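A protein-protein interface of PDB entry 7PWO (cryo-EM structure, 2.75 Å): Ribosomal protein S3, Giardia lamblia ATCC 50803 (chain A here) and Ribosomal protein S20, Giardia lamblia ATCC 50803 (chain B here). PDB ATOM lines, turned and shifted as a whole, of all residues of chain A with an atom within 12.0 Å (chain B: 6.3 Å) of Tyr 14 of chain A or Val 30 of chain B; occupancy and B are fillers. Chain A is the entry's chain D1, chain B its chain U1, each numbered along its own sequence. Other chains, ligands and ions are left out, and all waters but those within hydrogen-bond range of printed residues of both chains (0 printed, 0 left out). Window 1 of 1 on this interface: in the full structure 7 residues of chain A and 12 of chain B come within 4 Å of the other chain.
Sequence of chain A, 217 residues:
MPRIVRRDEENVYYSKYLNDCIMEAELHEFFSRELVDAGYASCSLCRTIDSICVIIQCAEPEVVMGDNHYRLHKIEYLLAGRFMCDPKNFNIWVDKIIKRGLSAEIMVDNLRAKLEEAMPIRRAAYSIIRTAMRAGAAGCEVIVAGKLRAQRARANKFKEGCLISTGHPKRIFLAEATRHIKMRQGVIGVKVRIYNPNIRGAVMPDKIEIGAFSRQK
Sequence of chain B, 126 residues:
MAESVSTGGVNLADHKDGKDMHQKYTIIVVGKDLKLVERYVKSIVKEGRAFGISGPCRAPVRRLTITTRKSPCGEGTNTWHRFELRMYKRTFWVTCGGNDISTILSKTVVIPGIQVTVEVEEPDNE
OH of Tyr 14 of chain A sits at hydrogen-bond distance from O of Met 87 of chain B, 3.2 Å away. O of Tyr 88 of chain B is in hydrogen-bond range of OH of Tyr 14 of chain A, 3.0 Å away. The backbone carbonyl oxygen (O) of Gly 113 of chain B sits at hydrogen-bond distance from the side-chain hydroxyl (OH) of Tyr 17 of chain A (2.7 Å). The side-chain carboxylate of Asp 20 of chain A sits at hydrogen-bond distance from the side-chain amide nitrogen of Gln 115 of chain B (3.0 Å).
The backbone carbonyl oxygen (O) of Arg 62 of chain B sits at hydrogen-bond distance from the backbone NH (N) of Met 87 of chain B (3.2 Å). The backbone carbonyl oxygen (O) of Tyr 17 of chain A lies within hydrogen-bond range of the side-chain sulfur (SG) of Cys 21 of chain A (3.2 Å). N of Gln 115 of chain B lies within hydrogen-bond range of O of Val 30 of chain B (2.9 Å). O of Gly 31 of chain B lies close to N of Tyr 88 of chain B, at 3.5 Å.
Among the printed residues, pairs that only touch across the chains: Tyr 13 of chain A with Ile 28 of chain B (3.8 Å), Tyr 14 of chain A with Val 30 of chain B (3.3 Å), Tyr 14 of chain A with Arg 62 of chain B (3.0 Å), Tyr 14 of chain A with Lys 89 of chain B (2.9 Å), Tyr 17 of chain A with Lys 32 of chain B (3.8 Å), Tyr 17 of chain A with Met 87 of chain B (3.2 Å), Tyr 17 of chain A with Gln 115 of chain B (3.4 Å), Cys 21 of chain A with Lys 32 of chain B (3.999 Å) and Leu 45 of chain A with Gly 113 of chain B (3.8 Å).
Tyr 14 of chain A touches just these residues of chain B: Val 30 (3.3 Å), Arg 62 (3.0 Å), Met 87 (3.2 Å), Tyr 88 (3.0 Å) and Lys 89 (2.9 Å). Val 30 of chain B touches just one residue of chain A: Tyr 14 (3.3 Å). Ile 28 of chain B touches just one residue of chain A: Tyr 13 (3.8 Å). No residue of chain A comes within 4 Å of Val 37 of chain B. Arg 62 of chain B touches just one residue of chain A: Tyr 14 (3.0 Å). Lys 89 of chain B touches one residue of chain A. Of chain A, only Tyr 17 (2.7 Å) and Leu 45 (3.8 Å) come within 4 Å of Gly 113 of chain B. No residue of chain A comes within 4 Å of Ile 114 of chain B. Of the printed residues of chain A, Gln 115 of chain B touches Tyr 17 and Asp 20. Of the printed residues of chain A, Lys 32 of chain B touches Tyr 17 (3.8 Å) and Cys 21 (3.999 Å). Printed residues of chain A within 4 Å of Tyr 88 of chain B: Tyr 14 (3.0 Å). Printed residues of chain B within 4 Å of Asp 20 of chain A: Gln 115 (3.0 Å). Pro 60 of chain B touches none of the printed residues of chain A. The nearest residue of chain A that does not touch Val 30 of chain B is Tyr 17 of chain A (4.9 Å).
Hydrophobic or aromatic side chains of chain A within 4 Å of the printed part of chain B: Tyr 13, Tyr 14 and Tyr 17. Among the printed residues, no Asp or Glu carboxylate lies within 4 Å of a Lys or Arg side-chain nitrogen of the other chain.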
ATOM      1  N   VAL A  12       0.526  10.627   5.424  1.00  0.00           N
ATOM      2  CA  VAL A  12      -0.411  11.738   5.509  1.00  0.00           C
ATOM      3  C   VAL A  12      -0.818  12.041   6.954  1.00  0.00           C
ATOM      4  O   VAL A  12      -1.784  11.488   7.478  1.00  0.00           O
ATOM      5  CB  VAL A  12      -1.657  11.472   4.663  1.00  0.00           C
ATOM      6  CG1 VAL A  12      -2.519  12.711   4.614  1.00  0.00           C
ATOM      7  CG2 VAL A  12      -1.255  11.043   3.266  1.00  0.00           C
ATOM      8  N   TYR A  13      -0.073  12.952   7.577  1.00  0.00           N
ATOM      9  CA  TYR A  13      -0.346  13.432   8.923  1.00  0.00           C
ATOM     10  C   TYR A  13      -0.804  14.878   8.926  1.00  0.00           C
ATOM     11  O   TYR A  13      -0.726  15.545   9.966  1.00  0.00           O
ATOM     12  CB  TYR A  13       0.897  13.288   9.800  1.00  0.00           C
ATOM     13  CG  TYR A  13       1.051  11.926  10.412  1.00  0.00           C
ATOM     14  CD1 TYR A  13      -0.019  11.293  11.028  1.00  0.00           C
ATOM     15  CD2 TYR A  13       2.265  11.272  10.372  1.00  0.00           C
ATOM     16  CE1 TYR A  13       0.122  10.037  11.589  1.00  0.00           C
ATOM     17  CE2 TYR A  13       2.418  10.020  10.922  1.00  0.00           C
ATOM     18  CZ  TYR A  13       1.345   9.408  11.530  1.00  0.00           C
ATOM     19  OH  TYR A  13       1.515   8.158  12.078  1.00  0.00           O
ATOM     20  N   TYR A  14      -1.275  15.377   7.778  1.00  0.00           N
ATOM     21  CA  TYR A  14      -1.384  16.808   7.565  1.00  0.00           C
ATOM     22  C   TYR A  14      -2.810  17.305   7.410  1.00  0.00           C
ATOM     23  O   TYR A  14      -3.050  18.500   7.601  1.00  0.00           O
ATOM     24  CB  TYR A  14      -0.569  17.202   6.330  1.00  0.00           C
ATOM     25  CG  TYR A  14       0.866  17.389   6.709  1.00  0.00           C
ATOM     26  CD1 TYR A  14       1.207  18.130   7.810  1.00  0.00           C
ATOM     27  CD2 TYR A  14       1.878  16.811   5.987  1.00  0.00           C
ATOM     28  CE1 TYR A  14       2.520  18.293   8.168  1.00  0.00           C
ATOM     29  CE2 TYR A  14       3.180  16.984   6.334  1.00  0.00           C
ATOM     30  CZ  TYR A  14       3.501  17.725   7.429  1.00  0.00           C
ATOM     31  OH  TYR A  14       4.809  17.906   7.798  1.00  0.00           O
ATOM     32  N   SER A  15      -3.751  16.424   7.067  1.00  0.00           N
ATOM     33  CA  SER A  15      -5.165  16.754   7.179  1.00  0.00           C
ATOM     34  C   SER A  15      -5.492  17.297   8.564  1.00  0.00           C
ATOM     35  O   SER A  15      -6.162  18.328   8.707  1.00  0.00           O
ATOM     36  CB  SER A  15      -5.988  15.504   6.896  1.00  0.00           C
ATOM     37  OG  SER A  15      -6.192  14.777   8.101  1.00  0.00           O
ATOM     38  N   LYS A  16      -5.025  16.596   9.596  1.00  0.00           N
ATOM     39  CA  LYS A  16      -5.255  16.998  10.978  1.00  0.00           C
ATOM     40  C   LYS A  16      -4.793  18.429  11.218  1.00  0.00           C
ATOM     41  O   LYS A  16      -5.545  19.274  11.732  1.00  0.00           O
ATOM     42  CB  LYS A  16      -4.511  16.025  11.902  1.00  0.00           C
ATOM     43  CG  LYS A  16      -5.246  14.716  12.201  1.00  0.00           C
ATOM     44  CD  LYS A  16      -5.253  13.769  11.012  1.00  0.00           C
ATOM     45  CE  LYS A  16      -3.883  13.214  10.699  1.00  0.00           C
ATOM     46  NZ  LYS A  16      -3.873  12.239   9.580  1.00  0.00           N
ATOM     47  N   TYR A  17      -3.568  18.735  10.797  1.00  0.00           N
ATOM     48  CA  TYR A  17      -2.990  20.024  11.138  1.00  0.00           C
ATOM     49  C   TYR A  17      -3.650  21.128  10.320  1.00  0.00           C
ATOM     50  O   TYR A  17      -3.885  22.232  10.824  1.00  0.00           O
ATOM     51  CB  TYR A  17      -1.492  20.025  10.849  1.00  0.00           C
ATOM     52  CG  TYR A  17      -0.791  21.263  11.348  1.00  0.00           C
ATOM     53  CD1 TYR A  17      -0.461  21.359  12.691  1.00  0.00           C
ATOM     54  CD2 TYR A  17      -0.589  22.376  10.552  1.00  0.00           C
ATOM     55  CE1 TYR A  17       0.173  22.455  13.203  1.00  0.00           C
ATOM     56  CE2 TYR A  17       0.044  23.517  11.071  1.00  0.00           C
ATOM     57  CZ  TYR A  17       0.415  23.540  12.410  1.00  0.00           C
ATOM     58  OH  TYR A  17       1.032  24.627  12.986  1.00  0.00           O
ATOM     59  N   LEU A  18      -3.932  20.845   9.045  1.00  0.00           N
ATOM     60  CA  LEU A  18      -4.579  21.821   8.170  1.00  0.00           C
ATOM     61  C   LEU A  18      -5.966  22.187   8.678  1.00  0.00           C
ATOM     62  O   LEU A  18      -6.359  23.364   8.656  1.00  0.00           O
ATOM     63  CB  LEU A  18      -4.657  21.255   6.751  1.00  0.00           C
ATOM     64  CG  LEU A  18      -5.072  22.171   5.600  1.00  0.00           C
ATOM     65  CD1 LEU A  18      -3.879  22.949   5.084  1.00  0.00           C
ATOM     66  CD2 LEU A  18      -5.718  21.363   4.488  1.00  0.00           C
ATOM     67  N   ASN A  19      -6.735  21.189   9.122  1.00  0.00           N
ATOM     68  CA  ASN A  19      -8.021  21.487   9.737  1.00  0.00           C
ATOM     69  C   ASN A  19      -7.848  22.276  11.029  1.00  0.00           C
ATOM     70  O   ASN A  19      -8.676  23.140  11.339  1.00  0.00           O
ATOM     71  CB  ASN A  19      -8.801  20.194   9.977  1.00  0.00           C
ATOM     72  CG  ASN A  19      -9.179  19.503   8.692  1.00  0.00           C
ATOM     73  OD1 ASN A  19      -8.560  19.727   7.650  1.00  0.00           O
ATOM     74  ND2 ASN A  19     -10.200  18.656   8.749  1.00  0.00           N
ATOM     75  N   ASP A  20      -6.781  22.017  11.788  1.00  0.00           N
ATOM     76  CA  ASP A  20      -6.502  22.897  12.924  1.00  0.00           C
ATOM     77  C   ASP A  20      -6.303  24.341  12.477  1.00  0.00           C
ATOM     78  O   ASP A  20      -6.804  25.265  13.123  1.00  0.00           O
ATOM     79  CB  ASP A  20      -5.299  22.404  13.731  1.00  0.00           C
ATOM     80  CG  ASP A  20      -5.592  21.120  14.489  1.00  0.00           C
ATOM     81  OD1 ASP A  20      -6.764  20.917  14.848  1.00  0.00           O
ATOM     82  OD2 ASP A  20      -4.665  20.339  14.774  1.00  0.00           O
ATOM     83  N   CYS A  21      -5.571  24.555  11.383  1.00  0.00           N
ATOM     84  CA  CYS A  21      -5.383  25.919  10.886  1.00  0.00           C
ATOM     85  C   CYS A  21      -6.710  26.562  10.491  1.00  0.00           C
ATOM     86  O   CYS A  21      -6.986  27.715  10.854  1.00  0.00           O
ATOM     87  CB  CYS A  21      -4.420  25.944   9.695  1.00  0.00           C
ATOM     88  SG  CYS A  21      -2.834  25.104   9.871  1.00  0.00           S
ATOM     89  N   ILE A  22      -7.553  25.837   9.752  1.00  0.00           N
ATOM     90  CA  ILE A  22      -8.792  26.461   9.283  1.00  0.00           C
ATOM     91  C   ILE A  22      -9.733  26.734  10.454  1.00  0.00           C
ATOM     92  O   ILE A  22     -10.476  27.725  10.452  1.00  0.00           O
ATOM     93  CB  ILE A  22      -9.477  25.635   8.180  1.00  0.00           C
ATOM     94  CG1 ILE A  22     -10.595  26.478   7.573  1.00  0.00           C
ATOM     95  CG2 ILE A  22     -10.086  24.354   8.722  1.00  0.00           C
ATOM     96  CD1 ILE A  22     -11.139  25.957   6.317  1.00  0.00           C
ATOM     97  N   MET A  23      -9.704  25.887  11.488  1.00  0.00           N
ATOM     98  CA  MET A  23     -10.523  26.152  12.667  1.00  0.00           C
ATOM     99  C   MET A  23      -9.950  27.274  13.533  1.00  0.00           C
ATOM    100  O   MET A  23     -10.711  27.983  14.197  1.00  0.00           O
ATOM    101  CB  MET A  23     -10.693  24.870  13.483  1.00  0.00           C
ATOM    102  CG  MET A  23      -9.552  24.557  14.432  1.00  0.00           C
ATOM    103  SD  MET A  23      -9.952  23.235  15.589  1.00  0.00           S
ATOM    104  CE  MET A  23     -11.465  23.852  16.316  1.00  0.00           C
ATOM    105  N   LEU A  45      -4.088  28.576  19.141  1.00  0.00           N
ATOM    106  CA  LEU A  45      -4.718  27.266  19.259  1.00  0.00           C
ATOM    107  C   LEU A  45      -3.696  26.226  19.696  1.00  0.00           C
ATOM    108  O   LEU A  45      -2.616  26.127  19.110  1.00  0.00           O
ATOM    109  CB  LEU A  45      -5.377  26.882  17.928  1.00  0.00           C
ATOM    110  CG  LEU A  45      -6.078  25.542  17.757  1.00  0.00           C
ATOM    111  CD1 LEU A  45      -7.352  25.739  16.952  1.00  0.00           C
ATOM    112  CD2 LEU A  45      -5.158  24.594  17.027  1.00  0.00           C
ATOM    113  N   CYS A  46      -4.049  25.449  20.718  1.00  0.00           N
ATOM    114  CA  CYS A  46      -3.123  24.508  21.347  1.00  0.00           C
ATOM    115  C   CYS A  46      -3.859  23.321  21.946  1.00  0.00           C
ATOM    116  O   CYS A  46      -5.082  23.337  22.080  1.00  0.00           O
ATOM    117  CB  CYS A  46      -2.296  25.210  22.434  1.00  0.00           C
ATOM    118  SG  CYS A  46      -0.780  24.331  22.923  1.00  0.00           S
ATOM    119  N   ILE B  28       6.066  11.298  16.276  1.00  0.00           N
ATOM    120  CA  ILE B  28       5.980  12.160  15.103  1.00  0.00           C
ATOM    121  C   ILE B  28       5.652  13.568  15.588  1.00  0.00           C
ATOM    122  O   ILE B  28       4.609  13.781  16.224  1.00  0.00           O
ATOM    123  CB  ILE B  28       4.921  11.661  14.110  1.00  0.00           C
ATOM    124  CG1 ILE B  28       5.116  10.168  13.811  1.00  0.00           C
ATOM    125  CG2 ILE B  28       4.956  12.484  12.828  1.00  0.00           C
ATOM    126  CD1 ILE B  28       6.407   9.847  13.103  1.00  0.00           C
ATOM    127  N   VAL B  29       6.533  14.523  15.287  1.00  0.00           N
ATOM    128  CA  VAL B  29       6.423  15.899  15.764  1.00  0.00           C
ATOM    129  C   VAL B  29       6.520  16.850  14.576  1.00  0.00           C
ATOM    130  O   VAL B  29       7.476  16.778  13.794  1.00  0.00           O
ATOM    131  CB  VAL B  29       7.487  16.221  16.829  1.00  0.00           C
ATOM    132  CG1 VAL B  29       7.282  15.340  18.039  1.00  0.00           C
ATOM    133  CG2 VAL B  29       8.878  15.985  16.292  1.00  0.00           C
ATOM    134  N   VAL B  30       5.527  17.727  14.435  1.00  0.00           N
ATOM    135  CA  VAL B  30       5.282  18.492  13.216  1.00  0.00           C
ATOM    136  C   VAL B  30       4.964  19.945  13.558  1.00  0.00           C
ATOM    137  O   VAL B  30       4.285  20.224  14.549  1.00  0.00           O
ATOM    138  CB  VAL B  30       4.128  17.855  12.413  1.00  0.00           C
ATOM    139  CG1 VAL B  30       3.782  18.690  11.215  1.00  0.00           C
ATOM    140  CG2 VAL B  30       4.516  16.466  11.967  1.00  0.00           C
ATOM    141  N   GLY B  31       5.457  20.870  12.742  1.00  0.00           N
ATOM    142  CA  GLY B  31       5.052  22.261  12.849  1.00  0.00           C
ATOM    143  C   GLY B  31       5.437  23.013  11.596  1.00  0.00           C
ATOM    144  O   GLY B  31       6.380  22.638  10.891  1.00  0.00           O
ATOM    145  N   LYS B  32       4.688  24.089  11.325  1.00  0.00           N
ATOM    146  CA  LYS B  32       4.907  24.889  10.121  1.00  0.00           C
ATOM    147  C   LYS B  32       6.072  25.866  10.231  1.00  0.00           C
ATOM    148  O   LYS B  32       6.723  26.144   9.215  1.00  0.00           O
ATOM    149  CB  LYS B  32       3.643  25.669   9.748  1.00  0.00           C
ATOM    150  CG  LYS B  32       3.304  26.817  10.675  1.00  0.00           C
ATOM    151  CD  LYS B  32       2.255  27.746  10.074  1.00  0.00           C
ATOM    152  CE  LYS B  32       0.920  27.048   9.865  1.00  0.00           C
ATOM    153  NZ  LYS B  32      -0.090  27.937   9.212  1.00  0.00           N
ATOM    154  N   VAL B  37       9.876  24.570  15.197  1.00  0.00           N
ATOM    155  CA  VAL B  37      10.174  23.144  15.051  1.00  0.00           C
ATOM    156  C   VAL B  37      11.600  22.845  15.498  1.00  0.00           C
ATOM    157  O   VAL B  37      11.856  21.864  16.210  1.00  0.00           O
ATOM    158  CB  VAL B  37       9.939  22.681  13.602  1.00  0.00           C
ATOM    159  CG1 VAL B  37      10.212  21.177  13.466  1.00  0.00           C
ATOM    160  CG2 VAL B  37       8.546  22.988  13.193  1.00  0.00           C
ATOM    161  N   TYR B  40      11.906  22.918  19.125  1.00  0.00           N
ATOM    162  CA  TYR B  40      11.226  21.825  19.805  1.00  0.00           C
ATOM    163  C   TYR B  40      12.069  20.558  19.757  1.00  0.00           C
ATOM    164  O   TYR B  40      12.187  19.837  20.760  1.00  0.00           O
ATOM    165  CB  TYR B  40       9.847  21.631  19.173  1.00  0.00           C
ATOM    166  CG  TYR B  40       9.042  20.460  19.679  1.00  0.00           C
ATOM    167  CD1 TYR B  40       8.819  20.278  21.040  1.00  0.00           C
ATOM    168  CD2 TYR B  40       8.457  19.564  18.792  1.00  0.00           C
ATOM    169  CE1 TYR B  40       8.060  19.216  21.506  1.00  0.00           C
ATOM    170  CE2 TYR B  40       7.697  18.506  19.248  1.00  0.00           C
ATOM    171  CZ  TYR B  40       7.504  18.329  20.604  1.00  0.00           C
ATOM    172  OH  TYR B  40       6.748  17.268  21.045  1.00  0.00           O
ATOM    173  N   PRO B  60      10.960  14.102   4.470  1.00  0.00           N
ATOM    174  CA  PRO B  60      11.438  15.460   4.216  1.00  0.00           C
ATOM    175  C   PRO B  60      10.280  16.445   4.162  1.00  0.00           C
ATOM    176  O   PRO B  60       9.123  16.109   4.409  1.00  0.00           O
ATOM    177  CB  PRO B  60      12.109  15.326   2.858  1.00  0.00           C
ATOM    178  CG  PRO B  60      11.284  14.280   2.151  1.00  0.00           C
ATOM    179  CD  PRO B  60      10.611  13.424   3.208  1.00  0.00           C
ATOM    180  N   ARG B  62       7.511  18.992   2.665  1.00  0.00           N
ATOM    181  CA  ARG B  62       6.673  19.180   1.494  1.00  0.00           C
ATOM    182  C   ARG B  62       5.787  20.388   1.735  1.00  0.00           C
ATOM    183  O   ARG B  62       5.555  20.802   2.873  1.00  0.00           O
ATOM    184  CB  ARG B  62       5.825  17.946   1.164  1.00  0.00           C
ATOM    185  CG  ARG B  62       4.786  17.550   2.190  1.00  0.00           C
ATOM    186  CD  ARG B  62       4.290  16.161   1.850  1.00  0.00           C
ATOM    187  NE  ARG B  62       3.103  15.701   2.571  1.00  0.00           N
ATOM    188  CZ  ARG B  62       1.957  16.367   2.691  1.00  0.00           C
ATOM    189  NH1 ARG B  62       1.782  17.554   2.119  1.00  0.00           N
ATOM    190  NH2 ARG B  62       0.951  15.817   3.358  1.00  0.00           N
ATOM    191  N   LEU B  64       2.501  23.180   0.504  1.00  0.00           N
ATOM    192  CA  LEU B  64       1.067  23.200   0.253  1.00  0.00           C
ATOM    193  C   LEU B  64       0.819  24.513  -0.491  1.00  0.00           C
ATOM    194  O   LEU B  64       0.881  25.586   0.122  1.00  0.00           O
ATOM    195  CB  LEU B  64       0.323  23.173   1.591  1.00  0.00           C
ATOM    196  CG  LEU B  64       0.047  21.904   2.432  1.00  0.00           C
ATOM    197  CD1 LEU B  64      -0.832  20.839   1.826  1.00  0.00           C
ATOM    198  CD2 LEU B  64       1.353  21.299   2.924  1.00  0.00           C
ATOM    199  N   MET B  87       5.598  22.563   5.503  1.00  0.00           N
ATOM    200  CA  MET B  87       5.492  22.023   6.852  1.00  0.00           C
ATOM    201  C   MET B  87       6.342  20.764   6.968  1.00  0.00           C
ATOM    202  O   MET B  87       6.451  19.997   6.011  1.00  0.00           O
ATOM    203  CB  MET B  87       4.050  21.724   7.219  1.00  0.00           C
ATOM    204  CG  MET B  87       3.103  22.885   6.972  1.00  0.00           C
ATOM    205  SD  MET B  87       1.467  22.454   7.556  1.00  0.00           S
ATOM    206  CE  MET B  87       1.989  21.371   8.870  1.00  0.00           C
ATOM    207  N   TYR B  88       6.896  20.529   8.156  1.00  0.00           N
ATOM    208  CA  TYR B  88       8.011  19.612   8.358  1.00  0.00           C
ATOM    209  C   TYR B  88       7.633  18.382   9.184  1.00  0.00           C
ATOM    210  O   TYR B  88       6.727  18.441  10.018  1.00  0.00           O
ATOM    211  CB  TYR B  88       9.172  20.361   9.023  1.00  0.00           C
ATOM    212  CG  TYR B  88       9.399  21.740   8.429  1.00  0.00           C
ATOM    213  CD1 TYR B  88      10.157  21.897   7.280  1.00  0.00           C
ATOM    214  CD2 TYR B  88       8.865  22.880   9.014  1.00  0.00           C
ATOM    215  CE1 TYR B  88      10.365  23.149   6.719  1.00  0.00           C
ATOM    216  CE2 TYR B  88       9.080  24.128   8.472  1.00  0.00           C
ATOM    217  CZ  TYR B  88       9.824  24.257   7.320  1.00  0.00           C
ATOM    218  OH  TYR B  88      10.040  25.497   6.770  1.00  0.00           O
ATOM    219  N   LYS B  89       8.336  17.267   8.939  1.00  0.00           N
ATOM    220  CA  LYS B  89       8.326  16.102   9.823  1.00  0.00           C
ATOM    221  C   LYS B  89       9.604  16.138  10.649  1.00  0.00           C
ATOM    222  O   LYS B  89      10.631  16.633  10.176  1.00  0.00           O
ATOM    223  CB  LYS B  89       8.335  14.751   9.095  1.00  0.00           C
ATOM    224  CG  LYS B  89       7.051  14.172   8.482  1.00  0.00           C
ATOM    225  CD  LYS B  89       6.667  14.910   7.199  1.00  0.00           C
ATOM    226  CE  LYS B  89       5.461  14.265   6.531  1.00  0.00           C
ATOM    227  NZ  LYS B  89       5.003  15.017   5.332  1.00  0.00           N
ATOM    228  N   ARG B  90       9.549  15.646  11.885  1.00  0.00           N
ATOM    229  CA  ARG B  90      10.754  15.179  12.564  1.00  0.00           C
ATOM    230  C   ARG B  90      10.460  13.793  13.119  1.00  0.00           C
ATOM    231  O   ARG B  90       9.461  13.607  13.817  1.00  0.00           O
ATOM    232  CB  ARG B  90      11.187  16.140  13.675  1.00  0.00           C
ATOM    233  CG  ARG B  90      11.547  17.510  13.110  1.00  0.00           C
ATOM    234  CD  ARG B  90      12.788  17.507  12.272  1.00  0.00           C
ATOM    235  NE  ARG B  90      13.133  18.855  11.849  1.00  0.00           N
ATOM    236  CZ  ARG B  90      12.698  19.403  10.721  1.00  0.00           C
ATOM    237  NH1 ARG B  90      11.879  18.721   9.929  1.00  0.00           N
ATOM    238  NH2 ARG B  90      13.049  20.635  10.397  1.00  0.00           N
ATOM    239  N   GLY B 113       1.012  25.279  18.372  1.00  0.00           N
ATOM    240  CA  GLY B 113       1.141  25.285  16.931  1.00  0.00           C
ATOM    241  C   GLY B 113       1.909  24.049  16.519  1.00  0.00           C
ATOM    242  O   GLY B 113       1.953  23.677  15.343  1.00  0.00           O
ATOM    243  N   ILE B 114       2.531  23.410  17.503  1.00  0.00           N
ATOM    244  CA  ILE B 114       3.218  22.145  17.287  1.00  0.00           C
ATOM    245  C   ILE B 114       2.229  21.003  17.474  1.00  0.00           C
ATOM    246  O   ILE B 114       1.352  21.045  18.344  1.00  0.00           O
ATOM    247  CB  ILE B 114       4.427  22.039  18.237  1.00  0.00           C
ATOM    248  CG1 ILE B 114       5.532  22.993  17.778  1.00  0.00           C
ATOM    249  CG2 ILE B 114       4.949  20.610  18.331  1.00  0.00           C
ATOM    250  CD1 ILE B 114       5.879  22.884  16.310  1.00  0.00           C
ATOM    251  N   GLN B 115       2.364  19.974  16.640  1.00  0.00           N
ATOM    252  CA  GLN B 115       1.452  18.842  16.584  1.00  0.00           C
ATOM    253  C   GLN B 115       2.247  17.564  16.812  1.00  0.00           C
ATOM    254  O   GLN B 115       3.362  17.423  16.309  1.00  0.00           O
ATOM    255  CB  GLN B 115       0.739  18.792  15.223  1.00  0.00           C
ATOM    256  CG  GLN B 115      -0.484  17.893  15.159  1.00  0.00           C
ATOM    257  CD  GLN B 115      -1.779  18.673  15.305  1.00  0.00           C
ATOM    258  OE1 GLN B 115      -1.764  19.885  15.515  1.00  0.00           O
ATOM    259  NE2 GLN B 115      -2.906  17.982  15.197  1.00  0.00           N
ATOM    260  N   VAL B 116       1.684  16.637  17.575  1.00  0.00           N
ATOM    261  CA  VAL B 116       2.384  15.406  17.921  1.00  0.00           C
ATOM    262  C   VAL B 116       1.424  14.233  17.810  1.00  0.00           C
ATOM    263  O   VAL B 116       0.288  14.307  18.291  1.00  0.00           O
ATOM    264  CB  VAL B 116       2.990  15.463  19.336  1.00  0.00           C
ATOM    265  CG1 VAL B 116       3.611  14.126  19.693  1.00  0.00           C
ATOM    266  CG2 VAL B 116       4.028  16.570  19.429  1.00  0.00           C
